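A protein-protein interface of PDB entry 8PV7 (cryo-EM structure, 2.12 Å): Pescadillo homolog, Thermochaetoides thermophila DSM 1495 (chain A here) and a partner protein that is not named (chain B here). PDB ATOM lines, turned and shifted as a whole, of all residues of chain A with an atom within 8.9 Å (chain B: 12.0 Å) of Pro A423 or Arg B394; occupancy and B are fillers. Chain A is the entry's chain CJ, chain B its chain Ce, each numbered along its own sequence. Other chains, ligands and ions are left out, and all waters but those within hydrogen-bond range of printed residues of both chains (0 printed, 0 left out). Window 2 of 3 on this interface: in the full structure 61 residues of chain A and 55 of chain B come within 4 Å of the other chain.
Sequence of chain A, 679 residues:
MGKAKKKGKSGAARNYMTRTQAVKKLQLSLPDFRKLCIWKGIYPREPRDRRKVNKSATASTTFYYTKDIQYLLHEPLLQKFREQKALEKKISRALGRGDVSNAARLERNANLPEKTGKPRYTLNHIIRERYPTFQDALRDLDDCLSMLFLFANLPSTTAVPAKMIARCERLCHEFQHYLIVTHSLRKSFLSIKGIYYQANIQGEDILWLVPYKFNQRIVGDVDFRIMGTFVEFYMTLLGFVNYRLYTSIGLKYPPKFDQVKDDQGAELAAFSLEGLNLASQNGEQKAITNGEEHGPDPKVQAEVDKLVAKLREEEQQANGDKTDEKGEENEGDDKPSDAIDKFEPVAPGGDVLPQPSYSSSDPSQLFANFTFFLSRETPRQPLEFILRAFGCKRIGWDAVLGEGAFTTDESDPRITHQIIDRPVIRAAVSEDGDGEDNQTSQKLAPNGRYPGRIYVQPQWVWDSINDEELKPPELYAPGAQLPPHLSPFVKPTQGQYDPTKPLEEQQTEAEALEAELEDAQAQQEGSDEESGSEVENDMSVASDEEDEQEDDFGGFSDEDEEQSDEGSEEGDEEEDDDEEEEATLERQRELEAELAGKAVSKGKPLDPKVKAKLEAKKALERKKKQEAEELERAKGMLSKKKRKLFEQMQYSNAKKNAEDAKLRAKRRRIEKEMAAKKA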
ATOM      1  N   TYR A 212     -25.893   1.603  12.244  1.00  0.00           N
ATOM      2  CA  TYR A 212     -26.926   0.584  12.143  1.00  0.00           C
ATOM      3  C   TYR A 212     -28.054   0.909  13.113  1.00  0.00           C
ATOM      4  O   TYR A 212     -27.829   1.455  14.195  1.00  0.00           O
ATOM      5  CB  TYR A 212     -26.357  -0.795  12.460  1.00  0.00           C
ATOM      6  CG  TYR A 212     -25.368  -1.315  11.453  1.00  0.00           C
ATOM      7  CD1 TYR A 212     -25.785  -1.755  10.207  1.00  0.00           C
ATOM      8  CD2 TYR A 212     -24.017  -1.378  11.752  1.00  0.00           C
ATOM      9  CE1 TYR A 212     -24.885  -2.237   9.287  1.00  0.00           C
ATOM     10  CE2 TYR A 212     -23.111  -1.855  10.840  1.00  0.00           C
ATOM     11  CZ  TYR A 212     -23.549  -2.279   9.608  1.00  0.00           C
ATOM     12  OH  TYR A 212     -22.643  -2.758   8.698  1.00  0.00           O
ATOM     13  N   PHE A 214     -29.927   0.582  15.842  1.00  0.00           N
ATOM     14  CA  PHE A 214     -29.956  -0.071  17.140  1.00  0.00           C
ATOM     15  C   PHE A 214     -30.023   1.023  18.192  1.00  0.00           C
ATOM     16  O   PHE A 214     -30.012   2.213  17.874  1.00  0.00           O
ATOM     17  CB  PHE A 214     -28.732  -0.966  17.346  1.00  0.00           C
ATOM     18  CG  PHE A 214     -28.723  -2.185  16.480  1.00  0.00           C
ATOM     19  CD1 PHE A 214     -29.654  -3.187  16.666  1.00  0.00           C
ATOM     20  CD2 PHE A 214     -27.790  -2.327  15.469  1.00  0.00           C
ATOM     21  CE1 PHE A 214     -29.661  -4.306  15.865  1.00  0.00           C
ATOM     22  CE2 PHE A 214     -27.785  -3.448  14.668  1.00  0.00           C
ATOM     23  CZ  PHE A 214     -28.723  -4.439  14.867  1.00  0.00           C
ATOM     24  N   ARG A 376     -38.635  -8.908   6.797  1.00  0.00           N
ATOM     25  CA  ARG A 376     -38.701  -8.167   8.049  1.00  0.00           C
ATOM     26  C   ARG A 376     -37.320  -7.979   8.670  1.00  0.00           C
ATOM     27  O   ARG A 376     -37.018  -6.917   9.224  1.00  0.00           O
ATOM     28  CB  ARG A 376     -39.645  -8.902   9.003  1.00  0.00           C
ATOM     29  CG  ARG A 376     -39.787  -8.285  10.357  1.00  0.00           C
ATOM     30  CD  ARG A 376     -41.063  -8.739  11.030  1.00  0.00           C
ATOM     31  NE  ARG A 376     -41.092 -10.173  11.285  1.00  0.00           N
ATOM     32  CZ  ARG A 376     -41.986 -11.007  10.772  1.00  0.00           C
ATOM     33  NH1 ARG A 376     -42.936 -10.584   9.957  1.00  0.00           N
ATOM     34  NH2 ARG A 376     -41.923 -12.296  11.086  1.00  0.00           N
ATOM     35  N   GLU A 377     -36.453  -8.984   8.547  1.00  0.00           N
ATOM     36  CA  GLU A 377     -35.169  -8.953   9.240  1.00  0.00           C
ATOM     37  C   GLU A 377     -34.127  -8.135   8.482  1.00  0.00           C
ATOM     38  O   GLU A 377     -33.026  -7.904   8.991  1.00  0.00           O
ATOM     39  CB  GLU A 377     -34.672 -10.381   9.459  1.00  0.00           C
ATOM     40  CG  GLU A 377     -34.404 -11.142   8.176  1.00  0.00           C
ATOM     41  CD  GLU A 377     -35.616 -11.877   7.645  1.00  0.00           C
ATOM     42  OE1 GLU A 377     -36.733 -11.635   8.147  1.00  0.00           O
ATOM     43  OE2 GLU A 377     -35.455 -12.691   6.715  1.00  0.00           O
ATOM     44  N   THR A 378     -34.440  -7.708   7.264  1.00  0.00           N
ATOM     45  CA  THR A 378     -33.482  -6.953   6.471  1.00  0.00           C
ATOM     46  C   THR A 378     -33.579  -5.455   6.778  1.00  0.00           C
ATOM     47  O   THR A 378     -34.653  -4.952   7.114  1.00  0.00           O
ATOM     48  CB  THR A 378     -33.721  -7.214   4.987  1.00  0.00           C
ATOM     49  OG1 THR A 378     -34.977  -6.652   4.597  1.00  0.00           O
ATOM     50  CG2 THR A 378     -33.730  -8.707   4.718  1.00  0.00           C
ATOM     51  N   PRO A 379     -32.455  -4.706   6.664  1.00  0.00           N
ATOM     52  CA  PRO A 379     -32.489  -3.272   7.001  1.00  0.00           C
ATOM     53  C   PRO A 379     -33.132  -2.387   5.937  1.00  0.00           C
ATOM     54  O   PRO A 379     -32.538  -2.076   4.890  1.00  0.00           O
ATOM     55  CB  PRO A 379     -31.009  -2.929   7.207  1.00  0.00           C
ATOM     56  CG  PRO A 379     -30.262  -3.927   6.423  1.00  0.00           C
ATOM     57  CD  PRO A 379     -31.098  -5.161   6.309  1.00  0.00           C
ATOM     58  N   ILE A 420     -33.498 -11.685   2.077  1.00  0.00           N
ATOM     59  CA  ILE A 420     -33.728 -12.459   3.292  1.00  0.00           C
ATOM     60  C   ILE A 420     -32.454 -12.472   4.130  1.00  0.00           C
ATOM     61  O   ILE A 420     -31.357 -12.267   3.602  1.00  0.00           O
ATOM     62  CB  ILE A 420     -34.231 -13.885   2.971  1.00  0.00           C
ATOM     63  CG1 ILE A 420     -33.567 -14.517   1.729  1.00  0.00           C
ATOM     64  CG2 ILE A 420     -35.736 -13.891   2.789  1.00  0.00           C
ATOM     65  CD1 ILE A 420     -32.075 -14.784   1.755  1.00  0.00           C
ATOM     66  N   ASP A 421     -32.606 -12.676   5.435  1.00  0.00           N
ATOM     67  CA  ASP A 421     -31.473 -12.865   6.332  1.00  0.00           C
ATOM     68  C   ASP A 421     -31.785 -13.842   7.458  1.00  0.00           C
ATOM     69  O   ASP A 421     -31.187 -13.746   8.533  1.00  0.00           O
ATOM     70  CB  ASP A 421     -31.013 -11.522   6.900  1.00  0.00           C
ATOM     71  CG  ASP A 421     -29.508 -11.439   7.056  1.00  0.00           C
ATOM     72  OD1 ASP A 421     -28.827 -12.457   6.824  1.00  0.00           O
ATOM     73  OD2 ASP A 421     -29.005 -10.354   7.408  1.00  0.00           O
ATOM     74  N   ARG A 422     -32.714 -14.768   7.241  1.00  0.00           N
ATOM     75  CA  ARG A 422     -33.190 -15.708   8.240  1.00  0.00           C
ATOM     76  C   ARG A 422     -32.655 -17.100   7.951  1.00  0.00           C
ATOM     77  O   ARG A 422     -32.643 -17.515   6.784  1.00  0.00           O
ATOM     78  CB  ARG A 422     -34.725 -15.726   8.247  1.00  0.00           C
ATOM     79  CG  ARG A 422     -35.355 -16.187   9.539  1.00  0.00           C
ATOM     80  CD  ARG A 422     -36.841 -15.917   9.565  1.00  0.00           C
ATOM     81  NE  ARG A 422     -37.130 -14.495   9.453  1.00  0.00           N
ATOM     82  CZ  ARG A 422     -37.690 -13.773  10.414  1.00  0.00           C
ATOM     83  NH1 ARG A 422     -38.015 -14.307  11.577  1.00  0.00           N
ATOM     84  NH2 ARG A 422     -37.923 -12.481  10.202  1.00  0.00           N
ATOM     85  N   PRO A 423     -32.202 -17.856   8.963  1.00  0.00           N
ATOM     86  CA  PRO A 423     -31.739 -19.217   8.688  1.00  0.00           C
ATOM     87  C   PRO A 423     -32.880 -20.222   8.641  1.00  0.00           C
ATOM     88  O   PRO A 423     -33.072 -20.851   7.602  1.00  0.00           O
ATOM     89  CB  PRO A 423     -30.800 -19.516   9.861  1.00  0.00           C
ATOM     90  CG  PRO A 423     -31.118 -18.493  10.922  1.00  0.00           C
ATOM     91  CD  PRO A 423     -32.146 -17.539  10.399  1.00  0.00           C
ATOM     92  N   ARG A 449     -40.253 -21.580  -0.851  1.00  0.00           N
ATOM     93  CA  ARG A 449     -39.756 -20.602  -1.809  1.00  0.00           C
ATOM     94  C   ARG A 449     -40.714 -20.539  -2.989  1.00  0.00           C
ATOM     95  O   ARG A 449     -41.058 -21.575  -3.567  1.00  0.00           O
ATOM     96  CB  ARG A 449     -38.351 -20.967  -2.283  1.00  0.00           C
ATOM     97  CG  ARG A 449     -37.393 -21.330  -1.167  1.00  0.00           C
ATOM     98  CD  ARG A 449     -36.550 -20.136  -0.742  1.00  0.00           C
ATOM     99  NE  ARG A 449     -35.244 -20.538  -0.233  1.00  0.00           N
ATOM    100  CZ  ARG A 449     -34.238 -20.975  -0.981  1.00  0.00           C
ATOM    101  NH1 ARG A 449     -34.323 -21.018  -2.301  1.00  0.00           N
ATOM    102  NH2 ARG A 449     -33.114 -21.368  -0.390  1.00  0.00           N
ATOM    103  N   GLN A 457     -29.211 -12.676   0.064  1.00  0.00           N
ATOM    104  CA  GLN A 457     -28.847 -11.976   1.279  1.00  0.00           C
ATOM    105  C   GLN A 457     -28.521 -10.518   0.954  1.00  0.00           C
ATOM    106  O   GLN A 457     -28.208 -10.194  -0.192  1.00  0.00           O
ATOM    107  CB  GLN A 457     -27.665 -12.679   1.941  1.00  0.00           C
ATOM    108  CG  GLN A 457     -27.919 -14.142   2.231  1.00  0.00           C
ATOM    109  CD  GLN A 457     -26.933 -14.714   3.220  1.00  0.00           C
ATOM    110  OE1 GLN A 457     -26.459 -14.015   4.111  1.00  0.00           O
ATOM    111  NE2 GLN A 457     -26.616 -15.991   3.068  1.00  0.00           N
ATOM    112  N   PRO A 458     -28.612  -9.613   1.944  1.00  0.00           N
ATOM    113  CA  PRO A 458     -28.462  -8.175   1.637  1.00  0.00           C
ATOM    114  C   PRO A 458     -27.114  -7.757   1.065  1.00  0.00           C
ATOM    115  O   PRO A 458     -27.044  -6.703   0.426  1.00  0.00           O
ATOM    116  CB  PRO A 458     -28.723  -7.496   2.992  1.00  0.00           C
ATOM    117  CG  PRO A 458     -28.847  -8.589   3.998  1.00  0.00           C
ATOM    118  CD  PRO A 458     -29.234  -9.810   3.264  1.00  0.00           C
ATOM    119  N   PRO A 478     -29.787 -18.037   0.478  1.00  0.00           N
ATOM    120  CA  PRO A 478     -30.011 -18.258   1.914  1.00  0.00           C
ATOM    121  C   PRO A 478     -29.264 -19.480   2.428  1.00  0.00           C
ATOM    122  O   PRO A 478     -29.312 -20.558   1.835  1.00  0.00           O
ATOM    123  CB  PRO A 478     -31.529 -18.450   2.016  1.00  0.00           C
ATOM    124  CG  PRO A 478     -32.076 -18.314   0.634  1.00  0.00           C
ATOM    125  CD  PRO A 478     -31.035 -17.717  -0.230  1.00  0.00           C
ATOM    126  N   GLY A 479     -28.559 -19.297   3.542  1.00  0.00           N
ATOM    127  CA  GLY A 479     -27.772 -20.350   4.138  1.00  0.00           C
ATOM    128  C   GLY A 479     -26.386 -20.521   3.559  1.00  0.00           C
ATOM    129  O   GLY A 479     -25.612 -21.333   4.080  1.00  0.00           O
ATOM    130  N   ALA A 480     -26.045 -19.784   2.507  1.00  0.00           N
ATOM    131  CA  ALA A 480     -24.744 -19.927   1.877  1.00  0.00           C
ATOM    132  C   ALA A 480     -23.707 -19.052   2.569  1.00  0.00           C
ATOM    133  O   ALA A 480     -24.023 -18.044   3.203  1.00  0.00           O
ATOM    134  CB  ALA A 480     -24.820 -19.565   0.394  1.00  0.00           C
ATOM    135  N   LEU A 482     -21.260 -16.295   2.398  1.00  0.00           N
ATOM    136  CA  LEU A 482     -21.166 -15.150   1.514  1.00  0.00           C
ATOM    137  C   LEU A 482     -19.717 -14.914   1.089  1.00  0.00           C
ATOM    138  O   LEU A 482     -18.785 -15.255   1.819  1.00  0.00           O
ATOM    139  CB  LEU A 482     -21.712 -13.904   2.203  1.00  0.00           C
ATOM    140  CG  LEU A 482     -23.218 -13.861   2.447  1.00  0.00           C
ATOM    141  CD1 LEU A 482     -23.618 -12.536   3.055  1.00  0.00           C
ATOM    142  CD2 LEU A 482     -23.973 -14.097   1.155  1.00  0.00           C
ATOM    143  N   TYR B 215     -17.610  -5.896   7.708  1.00  0.00           N
ATOM    144  CA  TYR B 215     -18.381  -6.808   8.546  1.00  0.00           C
ATOM    145  C   TYR B 215     -18.151  -8.259   8.147  1.00  0.00           C
ATOM    146  O   TYR B 215     -18.307  -9.162   8.975  1.00  0.00           O
ATOM    147  CB  TYR B 215     -19.871  -6.463   8.475  1.00  0.00           C
ATOM    148  CG  TYR B 215     -20.649  -7.248   7.438  1.00  0.00           C
ATOM    149  CD1 TYR B 215     -20.550  -6.940   6.088  1.00  0.00           C
ATOM    150  CD2 TYR B 215     -21.487  -8.294   7.808  1.00  0.00           C
ATOM    151  CE1 TYR B 215     -21.251  -7.650   5.142  1.00  0.00           C
ATOM    152  CE2 TYR B 215     -22.190  -9.010   6.865  1.00  0.00           C
ATOM    153  CZ  TYR B 215     -22.064  -8.686   5.534  1.00  0.00           C
ATOM    154  OH  TYR B 215     -22.766  -9.395   4.591  1.00  0.00           O
ATOM    155  N   ASN B 216     -17.798  -8.498   6.888  1.00  0.00           N
ATOM    156  CA  ASN B 216     -17.480  -9.826   6.372  1.00  0.00           C
ATOM    157  C   ASN B 216     -16.164  -9.674   5.624  1.00  0.00           C
ATOM    158  O   ASN B 216     -16.138  -9.610   4.388  1.00  0.00           O
ATOM    159  CB  ASN B 216     -18.605 -10.353   5.478  1.00  0.00           C
ATOM    160  CG  ASN B 216     -18.314 -11.723   4.919  1.00  0.00           C
ATOM    161  OD1 ASN B 216     -17.566 -12.501   5.504  1.00  0.00           O
ATOM    162  ND2 ASN B 216     -18.896 -12.023   3.769  1.00  0.00           N
ATOM    163  N   VAL B 384     -13.696  -7.657  15.542  1.00  0.00           N
ATOM    164  CA  VAL B 384     -14.463  -8.844  15.894  1.00  0.00           C
ATOM    165  C   VAL B 384     -13.486  -9.995  16.099  1.00  0.00           C
ATOM    166  O   VAL B 384     -12.724 -10.342  15.192  1.00  0.00           O
ATOM    167  CB  VAL B 384     -15.499  -9.176  14.813  1.00  0.00           C
ATOM    168  CG1 VAL B 384     -16.439 -10.263  15.291  1.00  0.00           C
ATOM    169  CG2 VAL B 384     -16.280  -7.935  14.434  1.00  0.00           C
ATOM    170  N   GLU B 388     -16.031 -14.663  17.997  1.00  0.00           N
ATOM    171  CA  GLU B 388     -17.244 -13.870  17.847  1.00  0.00           C
ATOM    172  C   GLU B 388     -17.623 -13.622  16.394  1.00  0.00           C
ATOM    173  O   GLU B 388     -18.557 -12.853  16.147  1.00  0.00           O
ATOM    174  CB  GLU B 388     -17.084 -12.526  18.555  1.00  0.00           C
ATOM    175  CG  GLU B 388     -16.387 -12.598  19.893  1.00  0.00           C
ATOM    176  CD  GLU B 388     -15.911 -11.238  20.364  1.00  0.00           C
ATOM    177  OE1 GLU B 388     -15.872 -10.302  19.538  1.00  0.00           O
ATOM    178  OE2 GLU B 388     -15.573 -11.105  21.559  1.00  0.00           O
ATOM    179  N   LEU B 389     -16.920 -14.225  15.438  1.00  0.00           N
ATOM    180  CA  LEU B 389     -17.200 -13.983  14.028  1.00  0.00           C
ATOM    181  C   LEU B 389     -18.536 -14.590  13.627  1.00  0.00           C
ATOM    182  O   LEU B 389     -18.838 -15.738  13.957  1.00  0.00           O
ATOM    183  CB  LEU B 389     -16.080 -14.565  13.165  1.00  0.00           C
ATOM    184  CG  LEU B 389     -14.789 -13.758  13.053  1.00  0.00           C
ATOM    185  CD1 LEU B 389     -13.783 -14.507  12.205  1.00  0.00           C
ATOM    186  CD2 LEU B 389     -15.066 -12.393  12.457  1.00  0.00           C
ATOM    187  N   GLU B 390     -19.333 -13.811  12.908  1.00  0.00           N
ATOM    188  CA  GLU B 390     -20.645 -14.235  12.449  1.00  0.00           C
ATOM    189  C   GLU B 390     -20.657 -14.345  10.931  1.00  0.00           C
ATOM    190  O   GLU B 390     -19.745 -13.889  10.240  1.00  0.00           O
ATOM    191  CB  GLU B 390     -21.728 -13.263  12.924  1.00  0.00           C
ATOM    192  CG  GLU B 390     -21.889 -13.220  14.428  1.00  0.00           C
ATOM    193  CD  GLU B 390     -22.641 -14.413  14.972  1.00  0.00           C
ATOM    194  OE1 GLU B 390     -23.323 -15.102  14.184  1.00  0.00           O
ATOM    195  OE2 GLU B 390     -22.555 -14.663  16.191  1.00  0.00           O
ATOM    196  N   ASP B 391     -21.716 -14.962  10.417  1.00  0.00           N
ATOM    197  CA  ASP B 391     -21.834 -15.238   8.995  1.00  0.00           C
ATOM    198  C   ASP B 391     -22.994 -14.509   8.334  1.00  0.00           C
ATOM    199  O   ASP B 391     -23.218 -14.697   7.135  1.00  0.00           O
ATOM    200  CB  ASP B 391     -21.976 -16.745   8.764  1.00  0.00           C
ATOM    201  CG  ASP B 391     -23.027 -17.369   9.653  1.00  0.00           C
ATOM    202  OD1 ASP B 391     -23.870 -18.131   9.134  1.00  0.00           O
ATOM    203  OD2 ASP B 391     -23.014 -17.097  10.871  1.00  0.00           O
ATOM    204  N   SER B 392     -23.735 -13.690   9.071  1.00  0.00           N
ATOM    205  CA  SER B 392     -24.868 -12.966   8.520  1.00  0.00           C
ATOM    206  C   SER B 392     -24.851 -11.527   9.012  1.00  0.00           C
ATOM    207  O   SER B 392     -24.265 -11.217  10.050  1.00  0.00           O
ATOM    208  CB  SER B 392     -26.195 -13.635   8.893  1.00  0.00           C
ATOM    209  OG  SER B 392     -26.504 -13.437  10.260  1.00  0.00           O
ATOM    210  N   LEU B 393     -25.499 -10.649   8.242  1.00  0.00           N
ATOM    211  CA  LEU B 393     -25.625  -9.254   8.649  1.00  0.00           C
ATOM    212  C   LEU B 393     -26.554  -9.109   9.847  1.00  0.00           C
ATOM    213  O   LEU B 393     -26.415  -8.172  10.640  1.00  0.00           O
ATOM    214  CB  LEU B 393     -26.125  -8.413   7.471  1.00  0.00           C
ATOM    215  CG  LEU B 393     -26.266  -6.900   7.670  1.00  0.00           C
ATOM    216  CD1 LEU B 393     -24.977  -6.293   8.199  1.00  0.00           C
ATOM    217  CD2 LEU B 393     -26.701  -6.218   6.388  1.00  0.00           C
ATOM    218  N   ARG B 394     -27.506 -10.033   9.994  1.00  0.00           N
ATOM    219  CA  ARG B 394     -28.468  -9.968  11.091  1.00  0.00           C
ATOM    220  C   ARG B 394     -27.788 -10.123  12.446  1.00  0.00           C
ATOM    221  O   ARG B 394     -28.104  -9.403  13.399  1.00  0.00           O
ATOM    222  CB  ARG B 394     -29.536 -11.042  10.897  1.00  0.00           C
ATOM    223  CG  ARG B 394     -30.643 -11.011  11.921  1.00  0.00           C
ATOM    224  CD  ARG B 394     -31.614 -12.152  11.704  1.00  0.00           C
ATOM    225  NE  ARG B 394     -30.930 -13.436  11.604  1.00  0.00           N
ATOM    226  CZ  ARG B 394     -30.548 -14.163  12.644  1.00  0.00           C
ATOM    227  NH1 ARG B 394     -30.767 -13.762  13.884  1.00  0.00           N
ATOM    228  NH2 ARG B 394     -29.934 -15.322  12.433  1.00  0.00           N
ATOM    229  N   ARG B 395     -26.836 -11.043  12.546  1.00  0.00           N
ATOM    230  CA  ARG B 395     -26.139 -11.312  13.795  1.00  0.00           C
ATOM    231  C   ARG B 395     -24.873 -10.485  13.956  1.00  0.00           C
ATOM    232  O   ARG B 395     -24.058 -10.794  14.829  1.00  0.00           O
ATOM    233  CB  ARG B 395     -25.807 -12.800  13.902  1.00  0.00           C
ATOM    234  CG  ARG B 395     -27.029 -13.691  13.937  1.00  0.00           C
ATOM    235  CD  ARG B 395     -26.701 -15.051  14.515  1.00  0.00           C
ATOM    236  NE  ARG B 395     -25.735 -14.965  15.603  1.00  0.00           N
ATOM    237  CZ  ARG B 395     -26.044 -15.018  16.891  1.00  0.00           C
ATOM    238  NH1 ARG B 395     -27.294 -15.146  17.296  1.00  0.00           N
ATOM    239  NH2 ARG B 395     -25.072 -14.942  17.794  1.00  0.00           N
ATOM    240  N   LEU B 396     -24.690  -9.454  13.137  1.00  0.00           N
ATOM    241  CA  LEU B 396     -23.535  -8.581  13.281  1.00  0.00           C
ATOM    242  C   LEU B 396     -23.634  -7.793  14.581  1.00  0.00           C
ATOM    243  O   LEU B 396     -24.690  -7.259  14.929  1.00  0.00           O
ATOM    244  CB  LEU B 396     -23.436  -7.646  12.067  1.00  0.00           C
ATOM    245  CG  LEU B 396     -22.401  -6.524  11.870  1.00  0.00           C
ATOM    246  CD1 LEU B 396     -22.846  -5.194  12.452  1.00  0.00           C
ATOM    247  CD2 LEU B 396     -21.026  -6.910  12.407  1.00  0.00           C
ATOM    248  N   LYS B 397     -22.517  -7.733  15.301  1.00  0.00           N
ATOM    249  CA  LYS B 397     -22.390  -7.042  16.580  1.00  0.00           C
ATOM    250  C   LYS B 397     -21.639  -5.750  16.306  1.00  0.00           C
ATOM    251  O   LYS B 397     -20.416  -5.776  16.109  1.00  0.00           O
ATOM    252  CB  LYS B 397     -21.620  -7.917  17.568  1.00  0.00           C
ATOM    253  CG  LYS B 397     -21.328  -7.288  18.911  1.00  0.00           C
ATOM    254  CD  LYS B 397     -22.415  -7.609  19.907  1.00  0.00           C
ATOM    255  CE  LYS B 397     -22.687  -9.111  19.948  1.00  0.00           C
ATOM    256  NZ  LYS B 397     -21.471  -9.888  20.313  1.00  0.00           N
ATOM    257  N   PRO B 398     -22.315  -4.602  16.252  1.00  0.00           N
ATOM    258  CA  PRO B 398     -21.625  -3.361  15.877  1.00  0.00           C
ATOM    259  C   PRO B 398     -20.616  -2.940  16.936  1.00  0.00           C
ATOM    260  O   PRO B 398     -20.839  -3.105  18.137  1.00  0.00           O
ATOM    261  CB  PRO B 398     -22.762  -2.344  15.736  1.00  0.00           C
ATOM    262  CG  PRO B 398     -23.933  -2.957  16.395  1.00  0.00           C
ATOM    263  CD  PRO B 398     -23.772  -4.426  16.339  1.00  0.00           C
ATOM    264  N   GLU B 399     -19.496  -2.398  16.480  1.00  0.00           N
ATOM    265  CA  GLU B 399     -18.368  -2.079  17.339  1.00  0.00           C
ATOM    266  C   GLU B 399     -18.156  -0.575  17.410  1.00  0.00           C
ATOM    267  O   GLU B 399     -18.506   0.166  16.489  1.00  0.00           O
ATOM    268  CB  GLU B 399     -17.086  -2.753  16.847  1.00  0.00           C
ATOM    269  CG  GLU B 399     -17.217  -4.243  16.650  1.00  0.00           C
ATOM    270  CD  GLU B 399     -16.533  -5.025  17.750  1.00  0.00           C
ATOM    271  OE1 GLU B 399     -17.019  -6.120  18.091  1.00  0.00           O
ATOM    272  OE2 GLU B 399     -15.510  -4.541  18.274  1.00  0.00           O
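Among the printed residues, merely in contact across the chains: Asp A421 with Leu B393 (3.5 Å), Asp A421 with Ser B392 (3.5 Å), Leu A482 with Tyr B215 (3.6 Å), Pro A423 with Arg B394 (3.7 Å), Tyr A212 with Leu B396 (3.7 Å), Leu A482 with Asn B216 (3.7 Å) and Pro A458 with Leu B393 (3.99 Å).
Of chain B, only Arg B394 comes within 4 Å of Pro A423.
No residue of chain B comes within 4 Å of Glu A377.
Asp A421 touches three residues of chain B.
No residue of chain B comes within 4 Å of Arg A422.
Of the printed residues of chain A, Ser B392 touches Asp A421.
Of the printed residues of chain B, Pro A458 touches Leu B393.
Of the printed residues of chain B, Tyr A212 touches Leu B396.
Of the printed residues of chain A, Leu B393 touches Asp A421 and Pro A458.
Of the printed residues of chain A, Leu B396 touches Tyr A212.
Of the 15 printed residues of chain B, 6 touch a printed residue of chain A.
Printed residues of chain B that touch a printed residue of chain A: Tyr B215, Asn B216, Ser B392, Leu B393, Arg B394 and Leu B396.
Hydrophobic or aromatic side chains of chain B within 4 Å of the printed part of chain A: Tyr B215, Leu B393 and Leu B396.
Of the 17 printed residues of chain A, 5 touch a printed residue of chain B.
Hydrophobic or aromatic side chains of chain A that line the printed part of chain B: Tyr A212, Pro A423, Pro A458 and Leu A482.
Among the printed residues, 8 pairs touch across the chains.
The side-chain hydroxyl (OG) of Ser B392 is in hydrogen-bond range of the backbone NH (N) of Arg B395 (3.3 Å).
The side-chain carboxylate (OE2) of Glu A377 lies within hydrogen-bond range of the backbone NH (N) of Asp A421.
The backbone NH of Arg B394 sits at hydrogen-bond distance from the side-chain carboxylate of Asp A421, at 3.0 Å.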
